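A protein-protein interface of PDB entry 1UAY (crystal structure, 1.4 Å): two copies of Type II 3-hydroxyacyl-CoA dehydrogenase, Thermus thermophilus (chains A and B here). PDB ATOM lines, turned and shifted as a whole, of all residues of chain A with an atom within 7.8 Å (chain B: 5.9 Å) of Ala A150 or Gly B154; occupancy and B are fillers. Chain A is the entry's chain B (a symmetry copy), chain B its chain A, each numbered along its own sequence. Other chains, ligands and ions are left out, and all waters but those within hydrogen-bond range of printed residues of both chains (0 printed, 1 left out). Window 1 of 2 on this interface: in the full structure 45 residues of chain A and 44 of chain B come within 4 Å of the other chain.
Ala A150 touches Gly B154, and with the chains exchanged Gly A154 touches Ala B150. Gly B153 touches its own counterpart, Gly A153. Gly A153 touches Ala B157, and with the chains exchanged Ala A157 touches Gly B153. Gly A154 touches its own counterpart, Gly B154. 10 positions are printed for both chains. Of the 11 pairs that touch across the chains among the printed residues, 8 have their exchanged pair printed and touching as well.
Of the 21 printed residues of chain A, 8 touch a printed residue of chain B. Printed residues of chain A that touch a printed residue of chain B: Leu A98, Ala A138, Ala A146, Ala A149, Ala A150, Gly A153, Gly A154 and Ala A157. Hydrophobic or aromatic side chains of chain A that line the printed part of chain B: Leu A98, Ala A146, Ala A149, Ala A150 and Ala A157.
Leu A98 touches Leu B102 (CD1 to CD2, 3.8 Å). O of Ala A138 touches CB of Ala B157, at 3.4 Å. Ala A146 touches Leu B158 (CB to CD1, 3.7 Å). Ala A150 touches Gly B154 (O to CA, 3.3 Å). Gly B153 touches Gly A153. Ala B157 touches Gly A153. CA of Gly A154 touches O of Ala B150, 3.3 Å away. Gly B154 touches Gly A154. Ala B149 touches Ala A157 (O to CB, 3.3 Å). Ala A157 touches Gly B153 (CB to CA, 3.7 Å).
Val A97 touches none of the printed residues of chain B. Of the printed residues of chain B, Ala A150 touches Gly B154. Of the printed residues of chain B, Gly A153 touches Gly B153 (3.7 Å) and Ala B157 (3.7 Å). Val A156 touches none of the printed residues of chain B. Printed residues of chain A within 4 Å of Ala B149: Ala A157. Of the printed residues of chain A, Ala B150 touches Gly A154. Gly B153 touches two residues of chain A. Of the printed residues of chain A, Ala B157 touches Ala A138 (3.4 Å), Ala A149 (3.4 Å) and Gly A153 (3.7 Å). The nearest printed residue of chain B that does not touch Ala A157 is Ala B150 (4.2 Å).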
ATOM      1  N   PHE A  94       9.862   0.510   3.991  1.00  0.00           N
ATOM      2  CA  PHE A  94       9.603   0.285   2.573  1.00  0.00           C
ATOM      3  C   PHE A  94       9.007   1.556   1.976  1.00  0.00           C
ATOM      4  O   PHE A  94       9.452   2.035   0.931  1.00  0.00           O
ATOM      5  CB  PHE A  94       8.617  -0.871   2.395  1.00  0.00           C
ATOM      6  CG  PHE A  94       8.245  -1.145   0.962  1.00  0.00           C
ATOM      7  CD1 PHE A  94       9.063  -1.921   0.148  1.00  0.00           C
ATOM      8  CD2 PHE A  94       7.072  -0.621   0.426  1.00  0.00           C
ATOM      9  CE1 PHE A  94       8.718  -2.171  -1.182  1.00  0.00           C
ATOM     10  CE2 PHE A  94       6.721  -0.864  -0.896  1.00  0.00           C
ATOM     11  CZ  PHE A  94       7.542  -1.640  -1.702  1.00  0.00           C
ATOM     12  N   VAL A  97      11.545   4.463   1.400  1.00  0.00           N
ATOM     13  CA  VAL A  97      12.401   4.260   0.238  1.00  0.00           C
ATOM     14  C   VAL A  97      11.622   4.578  -1.038  1.00  0.00           C
ATOM     15  O   VAL A  97      12.139   5.234  -1.945  1.00  0.00           O
ATOM     16  CB  VAL A  97      12.921   2.812   0.194  1.00  0.00           C
ATOM     17  CG1 VAL A  97      13.691   2.568  -1.093  1.00  0.00           C
ATOM     18  CG2 VAL A  97      13.814   2.557   1.401  1.00  0.00           C
ATOM     19  N   LEU A  98      10.375   4.127  -1.105  1.00  0.00           N
ATOM     20  CA  LEU A  98       9.549   4.400  -2.275  1.00  0.00           C
ATOM     21  C   LEU A  98       9.308   5.897  -2.413  1.00  0.00           C
ATOM     22  O   LEU A  98       9.404   6.455  -3.508  1.00  0.00           O
ATOM     23  CB  LEU A  98       8.193   3.703  -2.160  1.00  0.00           C
ATOM     24  CG  LEU A  98       8.089   2.188  -2.299  1.00  0.00           C
ATOM     25  CD1 LEU A  98       6.627   1.844  -2.541  1.00  0.00           C
ATOM     26  CD2 LEU A  98       8.938   1.690  -3.457  1.00  0.00           C
ATOM     27  N   ASN A 101      12.971   7.718  -3.372  1.00  0.00           N
ATOM     28  CA  ASN A 101      13.505   7.276  -4.652  1.00  0.00           C
ATOM     29  C   ASN A 101      12.564   7.316  -5.842  1.00  0.00           C
ATOM     30  O   ASN A 101      12.984   7.656  -6.947  1.00  0.00           O
ATOM     31  CB  ASN A 101      14.072   5.859  -4.527  1.00  0.00           C
ATOM     32  CG  ASN A 101      15.210   5.766  -3.532  1.00  0.00           C
ATOM     33  OD1 ASN A 101      15.696   6.778  -3.022  1.00  0.00           O
ATOM     34  ND2 ASN A 101      15.648   4.547  -3.256  1.00  0.00           N
ATOM     35  N   LEU A 102      11.302   6.962  -5.630  1.00  0.00           N
ATOM     36  CA  LEU A 102      10.354   6.945  -6.733  1.00  0.00           C
ATOM     37  C   LEU A 102       9.458   8.173  -6.774  1.00  0.00           C
ATOM     38  O   LEU A 102       9.453   8.902  -7.764  1.00  0.00           O
ATOM     39  CB  LEU A 102       9.510   5.661  -6.688  1.00  0.00           C
ATOM     40  CG  LEU A 102       8.464   5.470  -7.795  1.00  0.00           C
ATOM     41  CD1 LEU A 102       9.092   5.668  -9.170  1.00  0.00           C
ATOM     42  CD2 LEU A 102       7.864   4.075  -7.674  1.00  0.00           C
ATOM     43  N   ALA A 137      19.875  -2.605  -9.466  1.00  0.00           N
ATOM     44  CA  ALA A 137      19.052  -3.367  -8.526  1.00  0.00           C
ATOM     45  C   ALA A 137      17.633  -3.514  -9.076  1.00  0.00           C
ATOM     46  O   ALA A 137      16.886  -4.403  -8.663  1.00  0.00           O
ATOM     47  CB  ALA A 137      19.011  -2.676  -7.163  1.00  0.00           C
ATOM     48  N   ALA A 138      17.256  -2.634  -9.999  1.00  0.00           N
ATOM     49  CA  ALA A 138      15.931  -2.704 -10.601  1.00  0.00           C
ATOM     50  C   ALA A 138      15.809  -3.957 -11.466  1.00  0.00           C
ATOM     51  O   ALA A 138      14.701  -4.417 -11.754  1.00  0.00           O
ATOM     52  CB  ALA A 138      15.677  -1.465 -11.453  1.00  0.00           C
ATOM     53  N   GLY A 141      17.935  -7.420  -8.302  1.00  0.00           N
ATOM     54  CA  GLY A 141      17.945  -7.169  -6.872  1.00  0.00           C
ATOM     55  C   GLY A 141      18.468  -8.315  -6.025  1.00  0.00           C
ATOM     56  O   GLY A 141      18.065  -9.467  -6.195  1.00  0.00           O
ATOM     57  N   GLN A 145      17.406  -6.411  -0.727  1.00  0.00           N
ATOM     58  CA  GLN A 145      17.220  -5.177  -1.483  1.00  0.00           C
ATOM     59  C   GLN A 145      15.839  -5.041  -2.118  1.00  0.00           C
ATOM     60  O   GLN A 145      15.681  -4.344  -3.118  1.00  0.00           O
ATOM     61  CB  GLN A 145      18.297  -5.070  -2.570  1.00  0.00           C
ATOM     62  CG  GLN A 145      19.727  -4.967  -2.038  1.00  0.00           C
ATOM     63  CD  GLN A 145      19.963  -3.692  -1.242  1.00  0.00           C
ATOM     64  OE1 GLN A 145      19.764  -2.586  -1.747  1.00  0.00           O
ATOM     65  NE2 GLN A 145      20.394  -3.842   0.006  1.00  0.00           N
ATOM     66  N   ALA A 146      14.832  -5.680  -1.536  1.00  0.00           N
ATOM     67  CA  ALA A 146      13.489  -5.619  -2.097  1.00  0.00           C
ATOM     68  C   ALA A 146      12.925  -4.207  -2.190  1.00  0.00           C
ATOM     69  O   ALA A 146      12.386  -3.822  -3.226  1.00  0.00           O
ATOM     70  CB  ALA A 146      12.545  -6.504  -1.289  1.00  0.00           C
ATOM     71  N   ALA A 147      13.041  -3.433  -1.117  1.00  0.00           N
ATOM     72  CA  ALA A 147      12.509  -2.074  -1.116  1.00  0.00           C
ATOM     73  C   ALA A 147      13.239  -1.199  -2.124  1.00  0.00           C
ATOM     74  O   ALA A 147      12.617  -0.500  -2.925  1.00  0.00           O
ATOM     75  CB  ALA A 147      12.619  -1.468   0.277  1.00  0.00           C
ATOM     76  N   TYR A 148      14.564  -1.235  -2.078  1.00  0.00           N
ATOM     77  CA  TYR A 148      15.375  -0.439  -2.986  1.00  0.00           C
ATOM     78  C   TYR A 148      15.093  -0.833  -4.435  1.00  0.00           C
ATOM     79  O   TYR A 148      14.857   0.024  -5.285  1.00  0.00           O
ATOM     80  CB  TYR A 148      16.857  -0.633  -2.653  1.00  0.00           C
ATOM     81  CG  TYR A 148      17.791   0.272  -3.419  1.00  0.00           C
ATOM     82  CD1 TYR A 148      17.874   1.633  -3.126  1.00  0.00           C
ATOM     83  CD2 TYR A 148      18.600  -0.234  -4.430  1.00  0.00           C
ATOM     84  CE1 TYR A 148      18.748   2.466  -3.826  1.00  0.00           C
ATOM     85  CE2 TYR A 148      19.472   0.587  -5.133  1.00  0.00           C
ATOM     86  CZ  TYR A 148      19.541   1.932  -4.826  1.00  0.00           C
ATOM     87  OH  TYR A 148      20.414   2.739  -5.521  1.00  0.00           O
ATOM     88  N   ALA A 149      15.102  -2.132  -4.709  1.00  0.00           N
ATOM     89  CA  ALA A 149      14.844  -2.626  -6.057  1.00  0.00           C
ATOM     90  C   ALA A 149      13.486  -2.172  -6.571  1.00  0.00           C
ATOM     91  O   ALA A 149      13.360  -1.722  -7.710  1.00  0.00           O
ATOM     92  CB  ALA A 149      14.922  -4.149  -6.081  1.00  0.00           C
ATOM     93  N   ALA A 150      12.464  -2.295  -5.730  1.00  0.00           N
ATOM     94  CA  ALA A 150      11.119  -1.892  -6.121  1.00  0.00           C
ATOM     95  C   ALA A 150      11.074  -0.411  -6.484  1.00  0.00           C
ATOM     96  O   ALA A 150      10.488  -0.031  -7.498  1.00  0.00           O
ATOM     97  CB  ALA A 150      10.132  -2.191  -4.996  1.00  0.00           C
ATOM     98  N   SER A 151      11.707   0.426  -5.667  1.00  0.00           N
ATOM     99  CA  SER A 151      11.693   1.857  -5.932  1.00  0.00           C
ATOM    100  C   SER A 151      12.387   2.185  -7.248  1.00  0.00           C
ATOM    101  O   SER A 151      11.913   3.024  -8.015  1.00  0.00           O
ATOM    102  CB  SER A 151      12.358   2.635  -4.785  1.00  0.00           C
ATOM    103  OG  SER A 151      13.770   2.498  -4.781  1.00  0.00           O
ATOM    104  N   LYS A 152      13.496   1.508  -7.523  1.00  0.00           N
ATOM    105  CA  LYS A 152      14.236   1.771  -8.747  1.00  0.00           C
ATOM    106  C   LYS A 152      13.548   1.173  -9.971  1.00  0.00           C
ATOM    107  O   LYS A 152      13.672   1.707 -11.074  1.00  0.00           O
ATOM    108  CB  LYS A 152      15.675   1.268  -8.605  1.00  0.00           C
ATOM    109  CG  LYS A 152      16.448   1.962  -7.478  1.00  0.00           C
ATOM    110  CD  LYS A 152      16.535   3.465  -7.701  1.00  0.00           C
ATOM    111  CE  LYS A 152      17.423   4.139  -6.665  1.00  0.00           C
ATOM    112  NZ  LYS A 152      17.748   5.540  -7.055  1.00  0.00           N
ATOM    113  N   GLY A 153      12.818   0.076  -9.774  1.00  0.00           N
ATOM    114  CA  GLY A 153      12.089  -0.532 -10.874  1.00  0.00           C
ATOM    115  C   GLY A 153      10.985   0.422 -11.298  1.00  0.00           C
ATOM    116  O   GLY A 153      10.598   0.472 -12.464  1.00  0.00           O
ATOM    117  N   GLY A 154      10.465   1.181 -10.339  1.00  0.00           N
ATOM    118  CA  GLY A 154       9.431   2.148 -10.654  1.00  0.00           C
ATOM    119  C   GLY A 154      10.031   3.261 -11.495  1.00  0.00           C
ATOM    120  O   GLY A 154       9.406   3.743 -12.441  1.00  0.00           O
ATOM    121  N   VAL A 155      11.250   3.676 -11.159  1.00  0.00           N
ATOM    122  CA  VAL A 155      11.912   4.733 -11.917  1.00  0.00           C
ATOM    123  C   VAL A 155      12.151   4.247 -13.348  1.00  0.00           C
ATOM    124  O   VAL A 155      11.928   4.982 -14.311  1.00  0.00           O
ATOM    125  CB  VAL A 155      13.253   5.139 -11.256  1.00  0.00           C
ATOM    126  CG1 VAL A 155      13.992   6.140 -12.135  1.00  0.00           C
ATOM    127  CG2 VAL A 155      12.986   5.761  -9.887  1.00  0.00           C
ATOM    128  N   VAL A 156      12.589   3.000 -13.489  1.00  0.00           N
ATOM    129  CA  VAL A 156      12.825   2.431 -14.812  1.00  0.00           C
ATOM    130  C   VAL A 156      11.549   2.453 -15.654  1.00  0.00           C
ATOM    131  O   VAL A 156      11.560   2.928 -16.793  1.00  0.00           O
ATOM    132  CB  VAL A 156      13.333   0.973 -14.709  1.00  0.00           C
ATOM    133  CG1 VAL A 156      13.219   0.271 -16.064  1.00  0.00           C
ATOM    134  CG2 VAL A 156      14.780   0.967 -14.230  1.00  0.00           C
ATOM    135  N   ALA A 157      10.451   1.957 -15.089  1.00  0.00           N
ATOM    136  CA  ALA A 157       9.175   1.892 -15.799  1.00  0.00           C
ATOM    137  C   ALA A 157       8.570   3.249 -16.147  1.00  0.00           C
ATOM    138  O   ALA A 157       7.798   3.365 -17.099  1.00  0.00           O
ATOM    139  CB  ALA A 157       8.173   1.073 -14.985  1.00  0.00           C
ATOM    140  N   LEU B 102       1.698  -1.069  -5.495  1.00  0.00           N
ATOM    141  CA  LEU B 102       3.035  -1.502  -5.114  1.00  0.00           C
ATOM    142  C   LEU B 102       3.164  -1.795  -3.630  1.00  0.00           C
ATOM    143  O   LEU B 102       3.523  -2.907  -3.251  1.00  0.00           O
ATOM    144  CB  LEU B 102       4.062  -0.452  -5.555  1.00  0.00           C
ATOM    145  CG  LEU B 102       5.548  -0.715  -5.285  1.00  0.00           C
ATOM    146  CD1 LEU B 102       5.943  -2.117  -5.740  1.00  0.00           C
ATOM    147  CD2 LEU B 102       6.371   0.334  -6.015  1.00  0.00           C
ATOM    148  N   ALA B 149       2.256   2.692 -14.607  1.00  0.00           N
ATOM    149  CA  ALA B 149       3.464   2.015 -15.071  1.00  0.00           C
ATOM    150  C   ALA B 149       4.520   1.943 -13.971  1.00  0.00           C
ATOM    151  O   ALA B 149       5.140   0.896 -13.762  1.00  0.00           O
ATOM    152  CB  ALA B 149       4.029   2.737 -16.292  1.00  0.00           C
ATOM    153  N   ALA B 150       4.726   3.049 -13.265  1.00  0.00           N
ATOM    154  CA  ALA B 150       5.715   3.085 -12.197  1.00  0.00           C
ATOM    155  C   ALA B 150       5.370   2.075 -11.112  1.00  0.00           C
ATOM    156  O   ALA B 150       6.238   1.339 -10.640  1.00  0.00           O
ATOM    157  CB  ALA B 150       5.796   4.485 -11.600  1.00  0.00           C
ATOM    158  N   SER B 151       4.101   2.029 -10.719  1.00  0.00           N
ATOM    159  CA  SER B 151       3.695   1.100  -9.671  1.00  0.00           C
ATOM    160  C   SER B 151       3.907  -0.351 -10.094  1.00  0.00           C
ATOM    161  O   SER B 151       4.369  -1.171  -9.301  1.00  0.00           O
ATOM    162  CB  SER B 151       2.227   1.335  -9.277  1.00  0.00           C
ATOM    163  OG  SER B 151       1.319   0.855 -10.256  1.00  0.00           O
ATOM    164  N   LYS B 152       3.590  -0.664 -11.346  1.00  0.00           N
ATOM    165  CA  LYS B 152       3.741  -2.025 -11.843  1.00  0.00           C
ATOM    166  C   LYS B 152       5.208  -2.378 -12.082  1.00  0.00           C
ATOM    167  O   LYS B 152       5.600  -3.537 -11.952  1.00  0.00           O
ATOM    168  CB  LYS B 152       2.906  -2.205 -13.110  1.00  0.00           C
ATOM    169  CG  LYS B 152       1.412  -1.994 -12.871  1.00  0.00           C
ATOM    170  CD  LYS B 152       0.883  -2.950 -11.810  1.00  0.00           C
ATOM    171  CE  LYS B 152      -0.632  -2.871 -11.685  1.00  0.00           C
ATOM    172  NZ  LYS B 152      -1.175  -3.968 -10.835  1.00  0.00           N
ATOM    173  N   GLY B 153       6.016  -1.378 -12.419  1.00  0.00           N
ATOM    174  CA  GLY B 153       7.436  -1.617 -12.612  1.00  0.00           C
ATOM    175  C   GLY B 153       8.055  -2.001 -11.276  1.00  0.00           C
ATOM    176  O   GLY B 153       9.006  -2.788 -11.215  1.00  0.00           O
ATOM    177  N   GLY B 154       7.521  -1.436 -10.198  1.00  0.00           N
ATOM    178  CA  GLY B 154       8.021  -1.757  -8.874  1.00  0.00           C
ATOM    179  C   GLY B 154       7.705  -3.203  -8.540  1.00  0.00           C
ATOM    180  O   GLY B 154       8.529  -3.908  -7.958  1.00  0.00           O
ATOM    181  N   VAL B 155       6.507  -3.649  -8.909  1.00  0.00           N
ATOM    182  CA  VAL B 155       6.104  -5.025  -8.650  1.00  0.00           C
ATOM    183  C   VAL B 155       7.023  -5.966  -9.430  1.00  0.00           C
ATOM    184  O   VAL B 155       7.484  -6.979  -8.902  1.00  0.00           O
ATOM    185  CB  VAL B 155       4.637  -5.265  -9.064  1.00  0.00           C
ATOM    186  CG1 VAL B 155       4.298  -6.739  -8.928  1.00  0.00           C
ATOM    187  CG2 VAL B 155       3.703  -4.434  -8.186  1.00  0.00           C
ATOM    188  N   VAL B 156       7.292  -5.625 -10.684  1.00  0.00           N
ATOM    189  CA  VAL B 156       8.175  -6.438 -11.511  1.00  0.00           C
ATOM    190  C   VAL B 156       9.557  -6.588 -10.871  1.00  0.00           C
ATOM    191  O   VAL B 156      10.072  -7.701 -10.750  1.00  0.00           O
ATOM    192  CB  VAL B 156       8.341  -5.817 -12.917  1.00  0.00           C
ATOM    193  CG1 VAL B 156       9.522  -6.453 -13.646  1.00  0.00           C
ATOM    194  CG2 VAL B 156       7.062  -6.012 -13.714  1.00  0.00           C
ATOM    195  N   ALA B 157      10.144  -5.471 -10.448  1.00  0.00           N
ATOM    196  CA  ALA B 157      11.477  -5.473  -9.848  1.00  0.00           C
ATOM    197  C   ALA B 157      11.550  -6.186  -8.501  1.00  0.00           C
ATOM    198  O   ALA B 157      12.613  -6.665  -8.107  1.00  0.00           O
ATOM    199  CB  ALA B 157      11.978  -4.039  -9.710  1.00  0.00           C
ATOM    200  N   LEU B 158      10.426  -6.248  -7.796  1.00  0.00           N
ATOM    201  CA  LEU B 158      10.360  -6.910  -6.497  1.00  0.00           C
ATOM    202  C   LEU B 158      10.482  -8.429  -6.621  1.00  0.00           C
ATOM    203  O   LEU B 158      11.003  -9.103  -5.727  1.00  0.00           O
ATOM    204  CB  LEU B 158       9.025  -6.568  -5.823  1.00  0.00           C
ATOM    205  CG  LEU B 158       8.626  -7.350  -4.572  1.00  0.00           C
ATOM    206  CD1 LEU B 158       9.631  -7.077  -3.463  1.00  0.00           C
ATOM    207  CD2 LEU B 158       7.222  -6.942  -4.136  1.00  0.00           C
ATOM    208  N   THR B 159      10.023  -8.959  -7.748  1.00  0.00           N
ATOM    209  CA  THR B 159      10.010 -10.399  -7.964  1.00  0.00           C
ATOM    210  C   THR B 159      11.294 -11.156  -7.644  1.00  0.00           C
ATOM    211  O   THR B 159      11.283 -12.083  -6.832  1.00  0.00           O
ATOM    212  CB  THR B 159       9.611 -10.744  -9.414  1.00  0.00           C
ATOM    213  OG1 THR B 159       8.534  -9.900  -9.834  1.00  0.00           O
ATOM    214  CG2 THR B 159       9.153 -12.194  -9.501  1.00  0.00           C
